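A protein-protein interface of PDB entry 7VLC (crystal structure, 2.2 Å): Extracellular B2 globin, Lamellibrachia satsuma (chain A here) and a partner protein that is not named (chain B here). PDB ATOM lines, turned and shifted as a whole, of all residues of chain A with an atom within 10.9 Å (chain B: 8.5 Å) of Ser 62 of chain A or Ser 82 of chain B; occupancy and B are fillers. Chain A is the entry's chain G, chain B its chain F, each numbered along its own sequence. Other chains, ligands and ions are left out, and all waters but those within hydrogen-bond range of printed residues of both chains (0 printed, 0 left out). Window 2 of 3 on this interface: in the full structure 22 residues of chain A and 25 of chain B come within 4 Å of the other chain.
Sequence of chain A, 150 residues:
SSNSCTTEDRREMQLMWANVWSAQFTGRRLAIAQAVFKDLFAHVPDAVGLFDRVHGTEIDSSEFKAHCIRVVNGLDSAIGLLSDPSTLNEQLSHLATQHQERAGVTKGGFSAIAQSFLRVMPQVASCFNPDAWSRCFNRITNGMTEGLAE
Printed residues of chain B that touch a printed residue of chain A: Leu 77, Ser 82, Val 83, Thr 86 and Gln 87. Hydrophobic or aromatic side chains of chain B that line the printed part of chain A: Leu 77 and Val 83. Of the 24 printed residues of chain A, 6 touch a printed residue of chain B. Printed residues of chain A that touch a printed residue of chain B: Thr 26, Ser 62, Lys 65, Ala 66, Ile 69 and Arg 70.
The side-chain hydroxyl (OG1) of Thr 86 of chain B is in hydrogen-bond range of the backbone carbonyl oxygen (O) of Ser 82 of chain B, at 2.8 Å. NZ of Lys 65 of chain A is in salt-bridge range of OD2 of Asp 60 of chain A.
Ser 62 of chain A touches two residues of chain B. No residue of chain B comes within 4 Å of Ser 61 of chain A. No residue of chain A comes within 4 Å of Glu 81 of chain B. No residue of chain A comes within 4 Å of Asn 85 of chain B. Printed residues of chain A within 4 Å of Thr 86 of chain B: Ser 62 (3.7 Å) and Ala 66 (3.7 Å). Of the printed residues of chain A, Leu 77 of chain B touches Thr 26 (3.6 Å) and Ile 69 (3.6 Å). Of the printed residues of chain B, Ala 66 of chain A touches Thr 86. Of the printed residues of chain B, Thr 26 of chain A touches Leu 77. Of the printed residues of chain B, Lys 65 of chain A touches Val 83 (3.8 Å). Printed residues of chain A within 4 Å of Gln 87 of chain B: Arg 70. The nearest residue of chain B that does not touch Ser 62 of chain A is Val 83 of chain B (4.3 Å). The nearest printed residue of chain A that does not touch Ser 82 of chain B is Glu 63 of chain A (6.7 Å).
Among the printed residues, merely in contact across the chains: Thr 26 of chain A with Leu 77 of chain B, Ile 69 of chain A with Leu 77 of chain B, Ala 66 of chain A with Thr 86 of chain B, Ser 62 of chain A with Thr 86 of chain B and Lys 65 of chain A with Val 83 of chain B.
OG of Ser 82 of chain B sits at hydrogen-bond distance from OG of Ser 62 of chain A (2.6 Å). OE1 of Gln 87 of chain B is in hydrogen-bond range of NH1 of Arg 70 of chain A.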
ATOM      1  N   THR A  26      15.007  -3.082 -15.170  1.00  0.00           N
ATOM      2  CA  THR A  26      14.750  -1.825 -15.857  1.00  0.00           C
ATOM      3  C   THR A  26      13.335  -1.310 -15.647  1.00  0.00           C
ATOM      4  O   THR A  26      13.034  -0.200 -16.099  1.00  0.00           O
ATOM      5  CB  THR A  26      15.004  -1.983 -17.357  1.00  0.00           C
ATOM      6  OG1 THR A  26      14.105  -2.960 -17.897  1.00  0.00           O
ATOM      7  CG2 THR A  26      16.430  -2.431 -17.600  1.00  0.00           C
ATOM      8  N   LEU A  30      12.886   2.413 -16.604  1.00  0.00           N
ATOM      9  CA  LEU A  30      12.156   2.681 -17.839  1.00  0.00           C
ATOM     10  C   LEU A  30      11.018   3.663 -17.604  1.00  0.00           C
ATOM     11  O   LEU A  30      10.760   4.534 -18.440  1.00  0.00           O
ATOM     12  CB  LEU A  30      11.629   1.368 -18.422  1.00  0.00           C
ATOM     13  CG  LEU A  30      11.501   1.250 -19.938  1.00  0.00           C
ATOM     14  CD1 LEU A  30      12.669   1.932 -20.626  1.00  0.00           C
ATOM     15  CD2 LEU A  30      11.438  -0.216 -20.333  1.00  0.00           C
ATOM     16  N   GLN A  34      10.750   7.264 -19.514  1.00  0.00           N
ATOM     17  CA  GLN A  34       9.557   7.466 -20.332  1.00  0.00           C
ATOM     18  C   GLN A  34       8.768   8.678 -19.861  1.00  0.00           C
ATOM     19  O   GLN A  34       8.325   9.495 -20.676  1.00  0.00           O
ATOM     20  CB  GLN A  34       8.679   6.216 -20.309  1.00  0.00           C
ATOM     21  CG  GLN A  34       9.191   5.081 -21.176  1.00  0.00           C
ATOM     22  CD  GLN A  34       8.350   3.827 -21.052  1.00  0.00           C
ATOM     23  OE1 GLN A  34       7.802   3.536 -19.991  1.00  0.00           O
ATOM     24  NE2 GLN A  34       8.241   3.076 -22.143  1.00  0.00           N
ATOM     25  N   PHE A  51      14.319  12.098 -32.564  1.00  0.00           N
ATOM     26  CA  PHE A  51      14.463  10.703 -32.174  1.00  0.00           C
ATOM     27  C   PHE A  51      13.768   9.780 -33.166  1.00  0.00           C
ATOM     28  O   PHE A  51      13.023   8.878 -32.768  1.00  0.00           O
ATOM     29  CB  PHE A  51      13.913  10.490 -30.761  1.00  0.00           C
ATOM     30  CG  PHE A  51      14.507  11.418 -29.738  1.00  0.00           C
ATOM     31  CD1 PHE A  51      15.737  11.137 -29.159  1.00  0.00           C
ATOM     32  CD2 PHE A  51      13.842  12.568 -29.358  1.00  0.00           C
ATOM     33  CE1 PHE A  51      16.289  11.989 -28.219  1.00  0.00           C
ATOM     34  CE2 PHE A  51      14.388  13.423 -28.421  1.00  0.00           C
ATOM     35  CZ  PHE A  51      15.614  13.132 -27.850  1.00  0.00           C
ATOM     36  N   ASP A  52      14.010   9.995 -34.460  1.00  0.00           N
ATOM     37  CA  ASP A  52      13.405   9.137 -35.473  1.00  0.00           C
ATOM     38  C   ASP A  52      14.068   7.767 -35.500  1.00  0.00           C
ATOM     39  O   ASP A  52      13.387   6.744 -35.644  1.00  0.00           O
ATOM     40  CB  ASP A  52      13.489   9.801 -36.849  1.00  0.00           C
ATOM     41  CG  ASP A  52      12.615  11.037 -36.956  1.00  0.00           C
ATOM     42  OD1 ASP A  52      11.818  11.290 -36.027  1.00  0.00           O
ATOM     43  OD2 ASP A  52      12.730  11.758 -37.972  1.00  0.00           O
ATOM     44  N   ARG A  53      15.396   7.728 -35.357  1.00  0.00           N
ATOM     45  CA  ARG A  53      16.110   6.458 -35.431  1.00  0.00           C
ATOM     46  C   ARG A  53      15.699   5.527 -34.299  1.00  0.00           C
ATOM     47  O   ARG A  53      15.586   4.312 -34.495  1.00  0.00           O
ATOM     48  CB  ARG A  53      17.620   6.699 -35.403  1.00  0.00           C
ATOM     49  CG  ARG A  53      18.443   5.480 -35.786  1.00  0.00           C
ATOM     50  CD  ARG A  53      19.921   5.698 -35.515  1.00  0.00           C
ATOM     51  NE  ARG A  53      20.229   5.632 -34.090  1.00  0.00           N
ATOM     52  CZ  ARG A  53      20.526   4.507 -33.452  1.00  0.00           C
ATOM     53  NH1 ARG A  53      20.799   4.528 -32.152  1.00  0.00           N
ATOM     54  NH2 ARG A  53      20.553   3.359 -34.114  1.00  0.00           N
ATOM     55  N   VAL A  54      15.464   6.078 -33.109  1.00  0.00           N
ATOM     56  CA  VAL A  54      15.056   5.290 -31.953  1.00  0.00           C
ATOM     57  C   VAL A  54      13.547   5.338 -31.734  1.00  0.00           C
ATOM     58  O   VAL A  54      13.070   4.971 -30.655  1.00  0.00           O
ATOM     59  CB  VAL A  54      15.812   5.731 -30.687  1.00  0.00           C
ATOM     60  CG1 VAL A  54      17.313   5.550 -30.874  1.00  0.00           C
ATOM     61  CG2 VAL A  54      15.486   7.177 -30.341  1.00  0.00           C
ATOM     62  N   HIS A  55      12.785   5.794 -32.732  1.00  0.00           N
ATOM     63  CA  HIS A  55      11.320   5.754 -32.723  1.00  0.00           C
ATOM     64  C   HIS A  55      10.742   6.603 -31.588  1.00  0.00           C
ATOM     65  O   HIS A  55       9.990   6.123 -30.736  1.00  0.00           O
ATOM     66  CB  HIS A  55      10.805   4.312 -32.640  1.00  0.00           C
ATOM     67  CG  HIS A  55      11.256   3.436 -33.768  1.00  0.00           C
ATOM     68  ND1 HIS A  55      10.555   2.319 -34.162  1.00  0.00           N
ATOM     69  CD2 HIS A  55      12.340   3.506 -34.578  1.00  0.00           C
ATOM     70  CE1 HIS A  55      11.183   1.738 -35.169  1.00  0.00           C
ATOM     71  NE2 HIS A  55      12.270   2.438 -35.440  1.00  0.00           N
ATOM     72  N   GLY A  56      11.095   7.888 -31.601  1.00  0.00           N
ATOM     73  CA  GLY A  56      10.575   8.808 -30.604  1.00  0.00           C
ATOM     74  C   GLY A  56       9.069   8.976 -30.644  1.00  0.00           C
ATOM     75  O   GLY A  56       8.474   9.392 -29.645  1.00  0.00           O
ATOM     76  N   THR A  57       8.437   8.660 -31.777  1.00  0.00           N
ATOM     77  CA  THR A  57       6.986   8.775 -31.879  1.00  0.00           C
ATOM     78  C   THR A  57       6.269   7.639 -31.160  1.00  0.00           C
ATOM     79  O   THR A  57       5.118   7.807 -30.742  1.00  0.00           O
ATOM     80  CB  THR A  57       6.560   8.811 -33.349  1.00  0.00           C
ATOM     81  OG1 THR A  57       6.931   7.583 -33.989  1.00  0.00           O
ATOM     82  CG2 THR A  57       7.232   9.971 -34.067  1.00  0.00           C
ATOM     83  N   GLU A  58       6.919   6.490 -31.009  1.00  0.00           N
ATOM     84  CA  GLU A  58       6.358   5.349 -30.290  1.00  0.00           C
ATOM     85  C   GLU A  58       7.132   5.201 -28.982  1.00  0.00           C
ATOM     86  O   GLU A  58       8.218   4.614 -28.952  1.00  0.00           O
ATOM     87  CB  GLU A  58       6.419   4.082 -31.138  1.00  0.00           C
ATOM     88  CG  GLU A  58       5.838   2.847 -30.456  1.00  0.00           C
ATOM     89  CD  GLU A  58       4.378   3.012 -30.063  1.00  0.00           C
ATOM     90  OE1 GLU A  58       3.666   3.798 -30.724  1.00  0.00           O
ATOM     91  OE2 GLU A  58       3.943   2.353 -29.092  1.00  0.00           O
ATOM     92  N   ILE A  59       6.554   5.730 -27.900  1.00  0.00           N
ATOM     93  CA  ILE A  59       7.255   5.821 -26.623  1.00  0.00           C
ATOM     94  C   ILE A  59       7.514   4.443 -26.028  1.00  0.00           C
ATOM     95  O   ILE A  59       8.507   4.243 -25.317  1.00  0.00           O
ATOM     96  CB  ILE A  59       6.454   6.716 -25.657  1.00  0.00           C
ATOM     97  CG1 ILE A  59       6.117   8.046 -26.335  1.00  0.00           C
ATOM     98  CG2 ILE A  59       7.233   6.966 -24.371  1.00  0.00           C
ATOM     99  CD1 ILE A  59       5.037   8.844 -25.633  1.00  0.00           C
ATOM    100  N   ASP A  60       6.646   3.469 -26.305  1.00  0.00           N
ATOM    101  CA  ASP A  60       6.762   2.147 -25.703  1.00  0.00           C
ATOM    102  C   ASP A  60       7.290   1.098 -26.679  1.00  0.00           C
ATOM    103  O   ASP A  60       7.063  -0.099 -26.476  1.00  0.00           O
ATOM    104  CB  ASP A  60       5.417   1.710 -25.121  1.00  0.00           C
ATOM    105  CG  ASP A  60       5.576   0.830 -23.895  1.00  0.00           C
ATOM    106  OD1 ASP A  60       5.945   1.362 -22.824  1.00  0.00           O
ATOM    107  OD2 ASP A  60       5.345  -0.393 -24.004  1.00  0.00           O
ATOM    108  N   SER A  61       7.992   1.518 -27.728  1.00  0.00           N
ATOM    109  CA  SER A  61       8.644   0.563 -28.612  1.00  0.00           C
ATOM    110  C   SER A  61       9.974   0.106 -28.015  1.00  0.00           C
ATOM    111  O   SER A  61      10.584   0.792 -27.191  1.00  0.00           O
ATOM    112  CB  SER A  61       8.886   1.171 -29.993  1.00  0.00           C
ATOM    113  OG  SER A  61       9.876   2.182 -29.939  1.00  0.00           O
ATOM    114  N   SER A  62      10.425  -1.073 -28.451  1.00  0.00           N
ATOM    115  CA  SER A  62      11.690  -1.603 -27.951  1.00  0.00           C
ATOM    116  C   SER A  62      12.851  -0.686 -28.308  1.00  0.00           C
ATOM    117  O   SER A  62      13.792  -0.529 -27.521  1.00  0.00           O
ATOM    118  CB  SER A  62      11.930  -3.010 -28.497  1.00  0.00           C
ATOM    119  OG  SER A  62      10.889  -3.886 -28.103  1.00  0.00           O
ATOM    120  N   GLU A  63      12.798  -0.059 -29.484  1.00  0.00           N
ATOM    121  CA  GLU A  63      13.871   0.849 -29.878  1.00  0.00           C
ATOM    122  C   GLU A  63      13.928   2.068 -28.964  1.00  0.00           C
ATOM    123  O   GLU A  63      15.016   2.499 -28.565  1.00  0.00           O
ATOM    124  CB  GLU A  63      13.698   1.276 -31.335  1.00  0.00           C
ATOM    125  CG  GLU A  63      13.807   0.139 -32.346  1.00  0.00           C
ATOM    126  CD  GLU A  63      12.512  -0.633 -32.503  1.00  0.00           C
ATOM    127  OE1 GLU A  63      11.506  -0.235 -31.878  1.00  0.00           O
ATOM    128  OE2 GLU A  63      12.498  -1.635 -33.251  1.00  0.00           O
ATOM    129  N   PHE A  64      12.771   2.637 -28.619  1.00  0.00           N
ATOM    130  CA  PHE A  64      12.769   3.799 -27.738  1.00  0.00           C
ATOM    131  C   PHE A  64      12.961   3.405 -26.281  1.00  0.00           C
ATOM    132  O   PHE A  64      13.518   4.192 -25.504  1.00  0.00           O
ATOM    133  CB  PHE A  64      11.476   4.596 -27.900  1.00  0.00           C
ATOM    134  CG  PHE A  64      11.508   5.933 -27.226  1.00  0.00           C
ATOM    135  CD1 PHE A  64      12.291   6.956 -27.732  1.00  0.00           C
ATOM    136  CD2 PHE A  64      10.766   6.171 -26.081  1.00  0.00           C
ATOM    137  CE1 PHE A  64      12.331   8.189 -27.114  1.00  0.00           C
ATOM    138  CE2 PHE A  64      10.799   7.406 -25.458  1.00  0.00           C
ATOM    139  CZ  PHE A  64      11.582   8.415 -25.976  1.00  0.00           C
ATOM    140  N   LYS A  65      12.509   2.210 -25.892  1.00  0.00           N
ATOM    141  CA  LYS A  65      12.834   1.695 -24.566  1.00  0.00           C
ATOM    142  C   LYS A  65      14.343   1.604 -24.381  1.00  0.00           C
ATOM    143  O   LYS A  65      14.882   2.026 -23.353  1.00  0.00           O
ATOM    144  CB  LYS A  65      12.194   0.321 -24.353  1.00  0.00           C
ATOM    145  CG  LYS A  65      10.704   0.342 -24.052  1.00  0.00           C
ATOM    146  CD  LYS A  65      10.179  -1.077 -23.911  1.00  0.00           C
ATOM    147  CE  LYS A  65       8.710  -1.101 -23.543  1.00  0.00           C
ATOM    148  NZ  LYS A  65       8.203  -2.496 -23.453  1.00  0.00           N
ATOM    149  N   ALA A  66      15.043   1.058 -25.380  1.00  0.00           N
ATOM    150  CA  ALA A  66      16.493   0.932 -25.288  1.00  0.00           C
ATOM    151  C   ALA A  66      17.159   2.297 -25.169  1.00  0.00           C
ATOM    152  O   ALA A  66      18.116   2.463 -24.402  1.00  0.00           O
ATOM    153  CB  ALA A  66      17.030   0.170 -26.498  1.00  0.00           C
ATOM    154  N   HIS A  67      16.662   3.291 -25.910  1.00  0.00           N
ATOM    155  CA  HIS A  67      17.207   4.640 -25.778  1.00  0.00           C
ATOM    156  C   HIS A  67      16.975   5.190 -24.376  1.00  0.00           C
ATOM    157  O   HIS A  67      17.882   5.779 -23.775  1.00  0.00           O
ATOM    158  CB  HIS A  67      16.594   5.574 -26.824  1.00  0.00           C
ATOM    159  CG  HIS A  67      17.023   7.002 -26.677  1.00  0.00           C
ATOM    160  ND1 HIS A  67      18.281   7.440 -27.030  1.00  0.00           N
ATOM    161  CD2 HIS A  67      16.368   8.085 -26.196  1.00  0.00           C
ATOM    162  CE1 HIS A  67      18.381   8.734 -26.781  1.00  0.00           C
ATOM    163  NE2 HIS A  67      17.234   9.149 -26.275  1.00  0.00           N
ATOM    164  N   CYS A  68      15.764   5.012 -23.843  1.00  0.00           N
ATOM    165  CA  CYS A  68      15.474   5.445 -22.479  1.00  0.00           C
ATOM    166  C   CYS A  68      16.436   4.811 -21.480  1.00  0.00           C
ATOM    167  O   CYS A  68      16.920   5.479 -20.559  1.00  0.00           O
ATOM    168  CB  CYS A  68      14.028   5.101 -22.120  1.00  0.00           C
ATOM    169  SG  CYS A  68      12.795   6.226 -22.810  1.00  0.00           S
ATOM    170  N   ILE A  69      16.734   3.526 -21.657  1.00  0.00           N
ATOM    171  CA  ILE A  69      17.665   2.850 -20.762  1.00  0.00           C
ATOM    172  C   ILE A  69      19.078   3.387 -20.957  1.00  0.00           C
ATOM    173  O   ILE A  69      19.832   3.556 -19.990  1.00  0.00           O
ATOM    174  CB  ILE A  69      17.578   1.329 -20.973  1.00  0.00           C
ATOM    175  CG1 ILE A  69      16.235   0.820 -20.443  1.00  0.00           C
ATOM    176  CG2 ILE A  69      18.744   0.611 -20.308  1.00  0.00           C
ATOM    177  CD1 ILE A  69      15.954  -0.620 -20.766  1.00  0.00           C
ATOM    178  N   ARG A  70      19.451   3.695 -22.202  1.00  0.00           N
ATOM    179  CA  ARG A  70      20.761   4.290 -22.444  1.00  0.00           C
ATOM    180  C   ARG A  70      20.877   5.678 -21.829  1.00  0.00           C
ATOM    181  O   ARG A  70      21.950   6.046 -21.339  1.00  0.00           O
ATOM    182  CB  ARG A  70      21.049   4.346 -23.947  1.00  0.00           C
ATOM    183  CG  ARG A  70      21.399   2.999 -24.560  1.00  0.00           C
ATOM    184  CD  ARG A  70      21.967   3.153 -25.968  1.00  0.00           C
ATOM    185  NE  ARG A  70      21.004   3.703 -26.921  1.00  0.00           N
ATOM    186  CZ  ARG A  70      20.151   2.971 -27.634  1.00  0.00           C
ATOM    187  NH1 ARG A  70      20.131   1.652 -27.496  1.00  0.00           N
ATOM    188  NH2 ARG A  70      19.316   3.557 -28.484  1.00  0.00           N
ATOM    189  N   VAL A  71      19.789   6.450 -21.825  1.00  0.00           N
ATOM    190  CA  VAL A  71      19.838   7.805 -21.281  1.00  0.00           C
ATOM    191  C   VAL A  71      20.044   7.770 -19.770  1.00  0.00           C
ATOM    192  O   VAL A  71      20.950   8.422 -19.238  1.00  0.00           O
ATOM    193  CB  VAL A  71      18.566   8.588 -21.659  1.00  0.00           C
ATOM    194  CG1 VAL A  71      18.525   9.925 -20.937  1.00  0.00           C
ATOM    195  CG2 VAL A  71      18.501   8.810 -23.160  1.00  0.00           C
ATOM    196  N   LEU B  77      18.502  -6.088 -18.345  1.00  0.00           N
ATOM    197  CA  LEU B  77      17.568  -6.436 -19.405  1.00  0.00           C
ATOM    198  C   LEU B  77      17.532  -7.929 -19.702  1.00  0.00           C
ATOM    199  O   LEU B  77      16.851  -8.341 -20.648  1.00  0.00           O
ATOM    200  CB  LEU B  77      17.909  -5.659 -20.679  1.00  0.00           C
ATOM    201  CG  LEU B  77      17.417  -4.216 -20.711  1.00  0.00           C
ATOM    202  CD1 LEU B  77      17.986  -3.481 -21.914  1.00  0.00           C
ATOM    203  CD2 LEU B  77      15.899  -4.206 -20.730  1.00  0.00           C
ATOM    204  N   LEU B  78      18.239  -8.748 -18.915  1.00  0.00           N
ATOM    205  CA  LEU B  78      18.259 -10.189 -19.156  1.00  0.00           C
ATOM    206  C   LEU B  78      16.874 -10.817 -19.085  1.00  0.00           C
ATOM    207  O   LEU B  78      16.664 -11.893 -19.655  1.00  0.00           O
ATOM    208  CB  LEU B  78      19.183 -10.881 -18.157  1.00  0.00           C
ATOM    209  CG  LEU B  78      20.685 -10.693 -18.379  1.00  0.00           C
ATOM    210  CD1 LEU B  78      21.471 -11.271 -17.210  1.00  0.00           C
ATOM    211  CD2 LEU B  78      21.114 -11.334 -19.694  1.00  0.00           C
ATOM    212  N   ASP B  79      15.929 -10.181 -18.396  1.00  0.00           N
ATOM    213  CA  ASP B  79      14.564 -10.681 -18.308  1.00  0.00           C
ATOM    214  C   ASP B  79      13.646 -10.082 -19.366  1.00  0.00           C
ATOM    215  O   ASP B  79      12.453 -10.401 -19.378  1.00  0.00           O
ATOM    216  CB  ASP B  79      13.984 -10.397 -16.917  1.00  0.00           C
ATOM    217  CG  ASP B  79      13.865  -8.911 -16.633  1.00  0.00           C
ATOM    218  OD1 ASP B  79      14.866  -8.190 -16.818  1.00  0.00           O
ATOM    219  OD2 ASP B  79      12.769  -8.459 -16.243  1.00  0.00           O
ATOM    220  N   ASP B  80      14.166  -9.222 -20.237  1.00  0.00           N
ATOM    221  CA  ASP B  80      13.385  -8.550 -21.274  1.00  0.00           C
ATOM    222  C   ASP B  80      14.040  -8.872 -22.615  1.00  0.00           C
ATOM    223  O   ASP B  80      14.860  -8.098 -23.115  1.00  0.00           O
ATOM    224  CB  ASP B  80      13.320  -7.049 -21.021  1.00  0.00           C
ATOM    225  CG  ASP B  80      12.158  -6.393 -21.727  1.00  0.00           C
ATOM    226  OD1 ASP B  80      11.648  -6.981 -22.703  1.00  0.00           O
ATOM    227  OD2 ASP B  80      11.752  -5.291 -21.303  1.00  0.00           O
ATOM    228  N   GLU B  81      13.662 -10.020 -23.188  1.00  0.00           N
ATOM    229  CA  GLU B  81      14.296 -10.520 -24.406  1.00  0.00           C
ATOM    230  C   GLU B  81      14.298  -9.479 -25.519  1.00  0.00           C
ATOM    231  O   GLU B  81      15.331  -9.227 -26.153  1.00  0.00           O
ATOM    232  CB  GLU B  81      13.581 -11.790 -24.870  1.00  0.00           C
ATOM    233  CG  GLU B  81      14.240 -13.068 -24.410  1.00  0.00           C
ATOM    234  CD  GLU B  81      15.612 -13.247 -25.018  1.00  0.00           C
ATOM    235  OE1 GLU B  81      15.736 -13.112 -26.256  1.00  0.00           O
ATOM    236  OE2 GLU B  81      16.567 -13.506 -24.258  1.00  0.00           O
ATOM    237  N   SER B  82      13.143  -8.863 -25.771  1.00  0.00           N
ATOM    238  CA  SER B  82      13.024  -7.912 -26.873  1.00  0.00           C
ATOM    239  C   SER B  82      13.966  -6.729 -26.689  1.00  0.00           C
ATOM    240  O   SER B  82      14.728  -6.378 -27.597  1.00  0.00           O
ATOM    241  CB  SER B  82      11.575  -7.436 -26.989  1.00  0.00           C
ATOM    242  OG  SER B  82      11.447  -6.396 -27.940  1.00  0.00           O
ATOM    243  N   VAL B  83      13.930  -6.101 -25.513  1.00  0.00           N
ATOM    244  CA  VAL B  83      14.757  -4.920 -25.289  1.00  0.00           C
ATOM    245  C   VAL B  83      16.218  -5.308 -25.095  1.00  0.00           C
ATOM    246  O   VAL B  83      17.121  -4.510 -25.378  1.00  0.00           O
ATOM    247  CB  VAL B  83      14.212  -4.116 -24.096  1.00  0.00           C
ATOM    248  CG1 VAL B  83      14.894  -2.758 -24.010  1.00  0.00           C
ATOM    249  CG2 VAL B  83      12.698  -3.962 -24.212  1.00  0.00           C
ATOM    250  N   LEU B  84      16.481  -6.528 -24.621  1.00  0.00           N
ATOM    251  CA  LEU B  84      17.862  -6.981 -24.481  1.00  0.00           C
ATOM    252  C   LEU B  84      18.551  -7.055 -25.837  1.00  0.00           C
ATOM    253  O   LEU B  84      19.641  -6.502 -26.027  1.00  0.00           O
ATOM    254  CB  LEU B  84      17.906  -8.341 -23.782  1.00  0.00           C
ATOM    255  CG  LEU B  84      19.242  -9.088 -23.832  1.00  0.00           C
ATOM    256  CD1 LEU B  84      20.311  -8.339 -23.054  1.00  0.00           C
ATOM    257  CD2 LEU B  84      19.100 -10.514 -23.321  1.00  0.00           C
ATOM    258  N   ASN B  85      17.922  -7.733 -26.799  1.00  0.00           N
ATOM    259  CA  ASN B  85      18.527  -7.876 -28.118  1.00  0.00           C
ATOM    260  C   ASN B  85      18.628  -6.536 -28.837  1.00  0.00           C
ATOM    261  O   ASN B  85      19.546  -6.336 -29.640  1.00  0.00           O
ATOM    262  CB  ASN B  85      17.731  -8.882 -28.948  1.00  0.00           C
ATOM    263  CG  ASN B  85      17.806 -10.288 -28.383  1.00  0.00           C
ATOM    264  OD1 ASN B  85      18.794 -10.664 -27.745  1.00  0.00           O
ATOM    265  ND2 ASN B  85      16.766 -11.077 -28.619  1.00  0.00           N
ATOM    266  N   THR B  86      17.705  -5.610 -28.558  1.00  0.00           N
ATOM    267  CA  THR B  86      17.832  -4.259 -29.095  1.00  0.00           C
ATOM    268  C   THR B  86      19.089  -3.580 -28.567  1.00  0.00           C
ATOM    269  O   THR B  86      19.836  -2.957 -29.330  1.00  0.00           O
ATOM    270  CB  THR B  86      16.593  -3.430 -28.746  1.00  0.00           C
ATOM    271  OG1 THR B  86      15.415  -4.115 -29.183  1.00  0.00           O
ATOM    272  CG2 THR B  86      16.650  -2.063 -29.417  1.00  0.00           C
ATOM    273  N   GLN B  87      19.341  -3.694 -27.260  1.00  0.00           N
ATOM    274  CA  GLN B  87      20.556  -3.119 -26.695  1.00  0.00           C
ATOM    275  C   GLN B  87      21.791  -3.897 -27.135  1.00  0.00           C
ATOM    276  O   GLN B  87      22.849  -3.305 -27.374  1.00  0.00           O
ATOM    277  CB  GLN B  87      20.458  -3.071 -25.169  1.00  0.00           C
ATOM    278  CG  GLN B  87      21.692  -2.500 -24.483  1.00  0.00           C
ATOM    279  CD  GLN B  87      21.976  -1.066 -24.888  1.00  0.00           C
ATOM    280  OE1 GLN B  87      21.062  -0.300 -25.188  1.00  0.00           O
ATOM    281  NE2 GLN B  87      23.253  -0.696 -24.902  1.00  0.00           N
ATOM    282  N   LEU B  88      21.673  -5.223 -27.254  1.00  0.00           N
ATOM    283  CA  LEU B  88      22.788  -6.016 -27.764  1.00  0.00           C
ATOM    284  C   LEU B  88      23.172  -5.595 -29.180  1.00  0.00           C
ATOM    285  O   LEU B  88      24.352  -5.657 -29.547  1.00  0.00           O
ATOM    286  CB  LEU B  88      22.441  -7.505 -27.727  1.00  0.00           C
ATOM    287  CG  LEU B  88      22.428  -8.196 -26.358  1.00  0.00           C
ATOM    288  CD1 LEU B  88      21.996  -9.646 -26.497  1.00  0.00           C
ATOM    289  CD2 LEU B  88      23.794  -8.105 -25.691  1.00  0.00           C
ATOM    290  N   ALA B  89      22.197  -5.157 -29.983  1.00  0.00           N
ATOM    291  CA  ALA B  89      22.508  -4.694 -31.330  1.00  0.00           C
ATOM    292  C   ALA B  89      23.141  -3.308 -31.311  1.00  0.00           C
ATOM    293  O   ALA B  89      23.976  -2.998 -32.168  1.00  0.00           O
ATOM    294  CB  ALA B  89      21.248  -4.703 -32.191  1.00  0.00           C
